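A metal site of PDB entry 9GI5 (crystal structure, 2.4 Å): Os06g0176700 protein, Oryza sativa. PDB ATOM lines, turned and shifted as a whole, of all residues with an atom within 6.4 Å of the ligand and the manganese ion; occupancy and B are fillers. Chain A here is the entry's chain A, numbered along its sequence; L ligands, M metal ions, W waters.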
ATOM      1  N   ARG A 210     -15.624 -19.871  26.331  1.00  0.00           N
ATOM      2  CA  ARG A 210     -15.711 -20.857  25.265  1.00  0.00           C
ATOM      3  C   ARG A 210     -17.133 -21.408  25.238  1.00  0.00           C
ATOM      4  O   ARG A 210     -17.516 -22.187  26.116  1.00  0.00           O
ATOM      5  CB  ARG A 210     -14.677 -21.974  25.465  1.00  0.00           C
ATOM      6  CG  ARG A 210     -14.569 -22.952  24.277  1.00  0.00           C
ATOM      7  CD  ARG A 210     -13.632 -24.126  24.589  1.00  0.00           C
ATOM      8  NE  ARG A 210     -13.632 -25.151  23.548  1.00  0.00           N
ATOM      9  CZ  ARG A 210     -12.672 -25.322  22.652  1.00  0.00           C
ATOM     10  NH1 ARG A 210     -11.603 -24.545  22.637  1.00  0.00           N
ATOM     11  NH2 ARG A 210     -12.784 -26.291  21.750  1.00  0.00           N
ATOM     12  N   ASN A 212     -19.312 -23.960  23.681  1.00  0.00           N
ATOM     13  CA  ASN A 212     -19.179 -25.195  22.937  1.00  0.00           C
ATOM     14  C   ASN A 212     -20.505 -25.600  22.331  1.00  0.00           C
ATOM     15  O   ASN A 212     -21.567 -25.465  22.958  1.00  0.00           O
ATOM     16  CB  ASN A 212     -18.666 -26.333  23.839  1.00  0.00           C
ATOM     17  CG  ASN A 212     -17.306 -26.039  24.404  1.00  0.00           C
ATOM     18  OD1 ASN A 212     -16.317 -25.944  23.674  1.00  0.00           O
ATOM     19  ND2 ASN A 212     -17.228 -25.913  25.735  1.00  0.00           N
ATOM     20  N   TYR A 214     -21.890 -29.065  20.652  1.00  0.00           N
ATOM     21  CA  TYR A 214     -21.667 -30.440  20.254  1.00  0.00           C
ATOM     22  C   TYR A 214     -22.874 -30.910  19.455  1.00  0.00           C
ATOM     23  O   TYR A 214     -23.932 -31.194  20.049  1.00  0.00           O
ATOM     24  CB  TYR A 214     -21.445 -31.336  21.473  1.00  0.00           C
ATOM     25  CG  TYR A 214     -20.432 -30.825  22.482  1.00  0.00           C
ATOM     26  CD1 TYR A 214     -20.817 -29.969  23.510  1.00  0.00           C
ATOM     27  CD2 TYR A 214     -19.105 -31.208  22.414  1.00  0.00           C
ATOM     28  CE1 TYR A 214     -19.907 -29.508  24.446  1.00  0.00           C
ATOM     29  CE2 TYR A 214     -18.170 -30.746  23.354  1.00  0.00           C
ATOM     30  CZ  TYR A 214     -18.590 -29.894  24.370  1.00  0.00           C
ATOM     31  OH  TYR A 214     -17.682 -29.432  25.297  1.00  0.00           O
ATOM     32  N   VAL A 226     -15.406 -33.476  22.508  1.00  0.00           N
ATOM     33  CA  VAL A 226     -14.095 -32.877  22.713  1.00  0.00           C
ATOM     34  C   VAL A 226     -13.159 -33.920  23.299  1.00  0.00           C
ATOM     35  O   VAL A 226     -13.546 -34.720  24.154  1.00  0.00           O
ATOM     36  CB  VAL A 226     -14.141 -31.605  23.594  1.00  0.00           C
ATOM     37  CG1 VAL A 226     -14.550 -31.917  25.025  1.00  0.00           C
ATOM     38  CG2 VAL A 226     -12.807 -30.872  23.538  1.00  0.00           C
ATOM     39  N   HIS A 229      -8.753 -34.238  27.898  1.00  0.00           N
ATOM     40  CA  HIS A 229      -7.809 -33.155  28.164  1.00  0.00           C
ATOM     41  C   HIS A 229      -8.026 -32.675  29.587  1.00  0.00           C
ATOM     42  O   HIS A 229      -9.102 -32.836  30.156  1.00  0.00           O
ATOM     43  CB  HIS A 229      -8.008 -32.000  27.174  1.00  0.00           C
ATOM     44  CG  HIS A 229      -9.276 -31.242  27.411  1.00  0.00           C
ATOM     45  ND1 HIS A 229     -10.507 -31.703  27.003  1.00  0.00           N
ATOM     46  CD2 HIS A 229      -9.499 -30.044  28.008  1.00  0.00           C
ATOM     47  CE1 HIS A 229     -11.436 -30.825  27.353  1.00  0.00           C
ATOM     48  NE2 HIS A 229     -10.854 -29.811  27.964  1.00  0.00           N
ATOM     49  N   SER A 230      -6.987 -32.061  30.133  1.00  0.00           N
ATOM     50  CA  SER A 230      -7.155 -31.190  31.294  1.00  0.00           C
ATOM     51  C   SER A 230      -7.105 -29.748  30.820  1.00  0.00           C
ATOM     52  O   SER A 230      -6.500 -29.438  29.785  1.00  0.00           O
ATOM     53  CB  SER A 230      -6.066 -31.437  32.339  1.00  0.00           C
ATOM     54  OG  SER A 230      -4.768 -31.311  31.782  1.00  0.00           O
ATOM     55  N   ASP A 231      -7.744 -28.869  31.573  1.00  0.00           N
ATOM     56  CA  ASP A 231      -7.723 -27.452  31.238  1.00  0.00           C
ATOM     57  C   ASP A 231      -6.361 -26.857  31.575  1.00  0.00           C
ATOM     58  O   ASP A 231      -5.670 -27.311  32.492  1.00  0.00           O
ATOM     59  CB  ASP A 231      -8.825 -26.707  31.992  1.00  0.00           C
ATOM     60  CG  ASP A 231     -10.231 -27.094  31.512  1.00  0.00           C
ATOM     61  OD1 ASP A 231     -10.339 -27.675  30.410  1.00  0.00           O
ATOM     62  OD2 ASP A 231     -11.216 -26.800  32.230  1.00  0.00           O
ATOM     63  N   THR A 236     -11.594 -23.372  36.036  1.00  0.00           N
ATOM     64  CA  THR A 236     -12.594 -23.318  34.979  1.00  0.00           C
ATOM     65  C   THR A 236     -13.971 -23.344  35.618  1.00  0.00           C
ATOM     66  O   THR A 236     -14.220 -24.141  36.532  1.00  0.00           O
ATOM     67  CB  THR A 236     -12.434 -24.495  34.006  1.00  0.00           C
ATOM     68  OG1 THR A 236     -11.131 -24.449  33.408  1.00  0.00           O
ATOM     69  CG2 THR A 236     -13.485 -24.441  32.932  1.00  0.00           C
ATOM     70  N   LEU A 238     -17.842 -23.878  34.528  1.00  0.00           N
ATOM     71  CA  LEU A 238     -18.564 -24.461  33.407  1.00  0.00           C
ATOM     72  C   LEU A 238     -20.056 -24.361  33.653  1.00  0.00           C
ATOM     73  O   LEU A 238     -20.535 -24.664  34.750  1.00  0.00           O
ATOM     74  CB  LEU A 238     -18.156 -25.924  33.212  1.00  0.00           C
ATOM     75  CG  LEU A 238     -18.894 -26.740  32.153  1.00  0.00           C
ATOM     76  CD1 LEU A 238     -18.662 -26.173  30.763  1.00  0.00           C
ATOM     77  CD2 LEU A 238     -18.464 -28.195  32.213  1.00  0.00           C
ATOM     78  N   VAL A 240     -23.768 -25.485  31.662  1.00  0.00           N
ATOM     79  CA  VAL A 240     -24.285 -26.372  30.622  1.00  0.00           C
ATOM     80  C   VAL A 240     -25.783 -26.169  30.477  1.00  0.00           C
ATOM     81  O   VAL A 240     -26.516 -26.132  31.477  1.00  0.00           O
ATOM     82  CB  VAL A 240     -23.970 -27.853  30.916  1.00  0.00           C
ATOM     83  CG1 VAL A 240     -24.315 -28.709  29.701  1.00  0.00           C
ATOM     84  CG2 VAL A 240     -22.497 -28.034  31.299  1.00  0.00           C
ATOM     85  N   ASP A 243     -28.046 -30.261  30.678  1.00  0.00           N
ATOM     86  CA  ASP A 243     -26.897 -31.098  30.318  1.00  0.00           C
ATOM     87  C   ASP A 243     -27.178 -32.338  29.482  1.00  0.00           C
ATOM     88  O   ASP A 243     -26.313 -32.750  28.700  1.00  0.00           O
ATOM     89  CB  ASP A 243     -26.157 -31.519  31.589  1.00  0.00           C
ATOM     90  CG  ASP A 243     -24.686 -31.767  31.333  1.00  0.00           C
ATOM     91  OD1 ASP A 243     -24.365 -32.429  30.321  1.00  0.00           O
ATOM     92  OD2 ASP A 243     -23.858 -31.292  32.126  1.00  0.00           O
ATOM     93  N   GLY A 246     -23.018 -36.318  28.657  1.00  0.00           N
ATOM     94  CA  GLY A 246     -21.892 -36.315  27.748  1.00  0.00           C
ATOM     95  C   GLY A 246     -20.558 -35.994  28.384  1.00  0.00           C
ATOM     96  O   GLY A 246     -19.516 -36.482  27.922  1.00  0.00           O
ATOM     97  N   LEU A 247     -20.554 -35.175  29.424  1.00  0.00           N
ATOM     98  CA  LEU A 247     -19.298 -34.870  30.099  1.00  0.00           C
ATOM     99  C   LEU A 247     -18.832 -36.087  30.880  1.00  0.00           C
ATOM    100  O   LEU A 247     -19.589 -36.662  31.667  1.00  0.00           O
ATOM    101  CB  LEU A 247     -19.455 -33.671  31.032  1.00  0.00           C
ATOM    102  CG  LEU A 247     -18.195 -33.312  31.827  1.00  0.00           C
ATOM    103  CD1 LEU A 247     -17.015 -33.066  30.898  1.00  0.00           C
ATOM    104  CD2 LEU A 247     -18.425 -32.114  32.748  1.00  0.00           C
ATOM    105  N   VAL A 260     -23.905 -31.942  34.705  1.00  0.00           N
ATOM    106  CA  VAL A 260     -23.905 -30.640  35.370  1.00  0.00           C
ATOM    107  C   VAL A 260     -25.357 -30.171  35.478  1.00  0.00           C
ATOM    108  O   VAL A 260     -25.944 -29.737  34.491  1.00  0.00           O
ATOM    109  CB  VAL A 260     -23.054 -29.615  34.616  1.00  0.00           C
ATOM    110  CG1 VAL A 260     -22.916 -28.334  35.441  1.00  0.00           C
ATOM    111  CG2 VAL A 260     -21.699 -30.195  34.272  1.00  0.00           C
ATOM    112  N   ASN A 268     -13.711 -26.840  37.967  1.00  0.00           N
ATOM    113  CA  ASN A 268     -12.613 -27.785  37.982  1.00  0.00           C
ATOM    114  C   ASN A 268     -11.285 -27.040  38.053  1.00  0.00           C
ATOM    115  O   ASN A 268     -11.158 -25.913  37.567  1.00  0.00           O
ATOM    116  CB  ASN A 268     -12.636 -28.726  36.779  1.00  0.00           C
ATOM    117  CG  ASN A 268     -12.481 -27.993  35.489  1.00  0.00           C
ATOM    118  OD1 ASN A 268     -13.413 -27.338  35.027  1.00  0.00           O
ATOM    119  ND2 ASN A 268     -11.300 -28.104  34.885  1.00  0.00           N
ATOM    120  N   HIS A 286     -10.749 -34.753  31.383  1.00  0.00           N
ATOM    121  CA  HIS A 286     -12.165 -34.886  31.129  1.00  0.00           C
ATOM    122  C   HIS A 286     -12.407 -34.851  29.628  1.00  0.00           C
ATOM    123  O   HIS A 286     -11.521 -34.475  28.850  1.00  0.00           O
ATOM    124  CB  HIS A 286     -12.960 -33.794  31.851  1.00  0.00           C
ATOM    125  CG  HIS A 286     -12.470 -32.409  31.590  1.00  0.00           C
ATOM    126  ND1 HIS A 286     -11.292 -31.923  32.108  1.00  0.00           N
ATOM    127  CD2 HIS A 286     -12.995 -31.405  30.833  1.00  0.00           C
ATOM    128  CE1 HIS A 286     -11.115 -30.673  31.706  1.00  0.00           C
ATOM    129  NE2 HIS A 286     -12.135 -30.336  30.923  1.00  0.00           N
ATOM    130  N   ARG A 287     -13.611 -35.238  29.220  1.00  0.00           N
ATOM    131  CA  ARG A 287     -13.942 -35.320  27.813  1.00  0.00           C
ATOM    132  C   ARG A 287     -15.458 -35.229  27.660  1.00  0.00           C
ATOM    133  O   ARG A 287     -16.211 -35.370  28.626  1.00  0.00           O
ATOM    134  CB  ARG A 287     -13.413 -36.612  27.180  1.00  0.00           C
ATOM    135  CG  ARG A 287     -14.261 -37.829  27.487  1.00  0.00           C
ATOM    136  CD  ARG A 287     -13.539 -39.121  27.188  1.00  0.00           C
ATOM    137  NE  ARG A 287     -14.358 -40.268  27.557  1.00  0.00           N
ATOM    138  CZ  ARG A 287     -13.965 -41.531  27.460  1.00  0.00           C
ATOM    139  NH1 ARG A 287     -12.757 -41.838  27.005  1.00  0.00           N
ATOM    140  NH2 ARG A 287     -14.803 -42.496  27.801  1.00  0.00           N
ATOM    141  N   VAL A 288     -15.895 -35.014  26.425  1.00  0.00           N
ATOM    142  CA  VAL A 288     -17.311 -34.998  26.082  1.00  0.00           C
ATOM    143  C   VAL A 288     -17.560 -36.002  24.973  1.00  0.00           C
ATOM    144  O   VAL A 288     -16.918 -35.945  23.912  1.00  0.00           O
ATOM    145  CB  VAL A 288     -17.786 -33.599  25.676  1.00  0.00           C
ATOM    146  CG1 VAL A 288     -19.247 -33.648  25.214  1.00  0.00           C
ATOM    147  CG2 VAL A 288     -17.629 -32.622  26.837  1.00  0.00           C
ATOM    148  N   ARG A 296     -25.653 -30.423  22.291  1.00  0.00           N
ATOM    149  CA  ARG A 296     -25.349 -30.068  23.661  1.00  0.00           C
ATOM    150  C   ARG A 296     -24.589 -28.746  23.636  1.00  0.00           C
ATOM    151  O   ARG A 296     -23.662 -28.587  22.835  1.00  0.00           O
ATOM    152  CB  ARG A 296     -24.528 -31.162  24.343  1.00  0.00           C
ATOM    153  CG  ARG A 296     -24.125 -30.896  25.772  1.00  0.00           C
ATOM    154  CD  ARG A 296     -23.456 -32.135  26.385  1.00  0.00           C
ATOM    155  NE  ARG A 296     -23.097 -31.922  27.788  1.00  0.00           N
ATOM    156  CZ  ARG A 296     -22.003 -31.289  28.187  1.00  0.00           C
ATOM    157  NH1 ARG A 296     -21.128 -30.804  27.319  1.00  0.00           N
ATOM    158  NH2 ARG A 296     -21.796 -31.110  29.491  1.00  0.00           N
ATOM    159  N   ILE A 297     -24.987 -27.822  24.498  1.00  0.00           N
ATOM    160  CA  ILE A 297     -24.391 -26.493  24.558  1.00  0.00           C
ATOM    161  C   ILE A 297     -23.836 -26.276  25.953  1.00  0.00           C
ATOM    162  O   ILE A 297     -24.506 -26.567  26.955  1.00  0.00           O
ATOM    163  CB  ILE A 297     -25.429 -25.400  24.211  1.00  0.00           C
ATOM    164  CG1 ILE A 297     -25.774 -25.445  22.718  1.00  0.00           C
ATOM    165  CG2 ILE A 297     -24.909 -24.031  24.605  1.00  0.00           C
ATOM    166  CD1 ILE A 297     -26.691 -24.310  22.272  1.00  0.00           C
ATOM    167  N   SER A 298     -22.599 -25.777  26.022  1.00  0.00           N
ATOM    168  CA  SER A 298     -22.014 -25.411  27.300  1.00  0.00           C
ATOM    169  C   SER A 298     -21.212 -24.126  27.137  1.00  0.00           C
ATOM    170  O   SER A 298     -20.808 -23.757  26.035  1.00  0.00           O
ATOM    171  CB  SER A 298     -21.127 -26.541  27.848  1.00  0.00           C
ATOM    172  OG  SER A 298     -19.906 -26.615  27.134  1.00  0.00           O
ATOM    173  N   LEU A 299     -21.009 -23.440  28.256  1.00  0.00           N
ATOM    174  CA  LEU A 299     -20.123 -22.288  28.306  1.00  0.00           C
ATOM    175  C   LEU A 299     -19.078 -22.532  29.383  1.00  0.00           C
ATOM    176  O   LEU A 299     -19.416 -22.840  30.526  1.00  0.00           O
ATOM    177  CB  LEU A 299     -20.897 -20.996  28.587  1.00  0.00           C
ATOM    178  CG  LEU A 299     -20.024 -19.810  29.038  1.00  0.00           C
ATOM    179  CD1 LEU A 299     -19.002 -19.463  27.962  1.00  0.00           C
ATOM    180  CD2 LEU A 299     -20.885 -18.590  29.375  1.00  0.00           C
ATOM    181  N   ALA A 300     -17.808 -22.395  29.011  1.00  0.00           N
ATOM    182  CA  ALA A 300     -16.697 -22.579  29.942  1.00  0.00           C
ATOM    183  C   ALA A 300     -15.911 -21.283  30.033  1.00  0.00           C
ATOM    184  O   ALA A 300     -15.420 -20.772  29.017  1.00  0.00           O
ATOM    185  CB  ALA A 300     -15.793 -23.727  29.498  1.00  0.00           C
ATOM    186  N   PHE A 302     -12.573 -19.852  31.269  1.00  0.00           N
ATOM    187  CA  PHE A 302     -11.227 -20.197  31.709  1.00  0.00           C
ATOM    188  C   PHE A 302     -10.559 -18.972  32.310  1.00  0.00           C
ATOM    189  O   PHE A 302     -10.535 -17.893  31.701  1.00  0.00           O
ATOM    190  CB  PHE A 302     -10.380 -20.725  30.546  1.00  0.00           C
ATOM    191  CG  PHE A 302     -11.010 -21.882  29.797  1.00  0.00           C
ATOM    192  CD1 PHE A 302     -11.154 -23.125  30.389  1.00  0.00           C
ATOM    193  CD2 PHE A 302     -11.444 -21.717  28.483  1.00  0.00           C
ATOM    194  CE1 PHE A 302     -11.727 -24.183  29.688  1.00  0.00           C
ATOM    195  CE2 PHE A 302     -12.018 -22.774  27.783  1.00  0.00           C
ATOM    196  CZ  PHE A 302     -12.153 -24.006  28.394  1.00  0.00           C
HETATM  197  C1  LIG L   1     -14.091 -27.103  27.704  1.00  0.00           C
HETATM  198  O1  LIG L   1     -14.683 -26.238  27.085  1.00  0.00           O
HETATM  199  O2  LIG L   1     -12.797 -27.124  27.890  1.00  0.00           O
HETATM  200  C2  LIG L   1     -14.848 -28.290  28.333  1.00  0.00           C
HETATM  201  O3  LIG L   1     -14.212 -29.194  28.875  1.00  0.00           O
HETATM  202  C3  LIG L   1     -16.354 -28.287  28.272  1.00  0.00           C
HETATM  203  C4  LIG L   1     -16.970 -29.556  28.836  1.00  0.00           C
HETATM  204  C5  LIG L   1     -18.473 -29.647  28.692  1.00  0.00           C
HETATM  205  O4  LIG L   1     -19.187 -30.133  29.539  1.00  0.00           O
HETATM  206  O5  LIG L   1     -18.927 -29.165  27.562  1.00  0.00           O
HETATM  207 MN    MN M   1     -12.059 -28.567  29.449  1.00  0.00          MN
HETATM  208  O   HOH W   1     -13.762 -27.584  31.335  1.00  0.00           O
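The side-chain carboxylate of Asp 231 is in hydrogen-bond range of the side-chain amide nitrogen of Asn 268, at 3.0 Å. OD2 of Asp 231 sits at hydrogen-bond distance from OG1 of Thr 236 (2.6 Å). The backbone NH (N) of Tyr 214 sits at hydrogen-bond distance from the backbone carbonyl oxygen (O) of Arg 296 (2.9 Å). The side-chain carboxylate of Asp 243 is in salt-bridge range of the guanidinium group of Arg 296. The backbone carbonyl oxygen (O) of Ser 298 lies within hydrogen-bond range of the backbone NH (N) of Asn 212. The guanidinium group (NE) of Arg 210 is in hydrogen-bond range of the side-chain amide oxygen (OD1) of Asn 212 (2.8 Å). O of Ala 300 sits at hydrogen-bond distance from N of Arg 210, at 2.8 Å. The backbone carbonyl oxygen of Val 288 sits at hydrogen-bond distance from the backbone NH of Val 226, at 3.2 Å.
Leu 238 touches the ligand. CD2 of Leu 247 touches O4 of the ligand, 3.8 Å away. Val 288 touches the ligand (CG2 to C5, 3.6 Å). Ala 300 touches the ligand (CB to O1, 3.7 Å). CZ of Phe 302 touches O2 of the ligand, 3.2 Å away. 13 residues have an atom within 4 Å of the ligand: Arg 210, Asn 212, Tyr 214, His 229, Asp 231, Leu 238, Leu 247, His 286, Val 288, Arg 296, Ser 298, Ala 300 and Phe 302. Along chain A the residues within 4 Å of the ligand span positions 210 to 302.
OH of Tyr 214 is in hydrogen-bond range of O5 of the ligand (2.6 Å). An oxygen (O5) of the ligand is in salt-bridge range of the guanidinium group (NH1) of Arg 296, at 2.8 Å. The side-chain hydroxyl (OG) of Ser 298 lies within hydrogen-bond range of an oxygen (O5) of the ligand, at 2.8 Å. The side-chain amide nitrogen (ND2) of Asn 212 lies within hydrogen-bond range of an oxygen (O1) of the ligand, at 2.9 Å. NE of Arg 210 lies within salt-bridge range of O1 of the ligand, 3.8 Å away.
The manganese ion is bound by OD1 of Asp 231 (2.2 Å), O2 of the ligand (2.2 Å), NE2 of His 229 (2.3 Å), NE2 of His 286 (2.3 Å) and O3 of the ligand (2.3 Å). Slightly farther from the manganese ion lies water W1 (2.7 Å).
Three residues have an atom within 4 Å of the manganese ion: His 229, Asp 231 and His 286. The nearest printed residue that does not touch the manganese ion is Phe 302 (4.4 Å).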
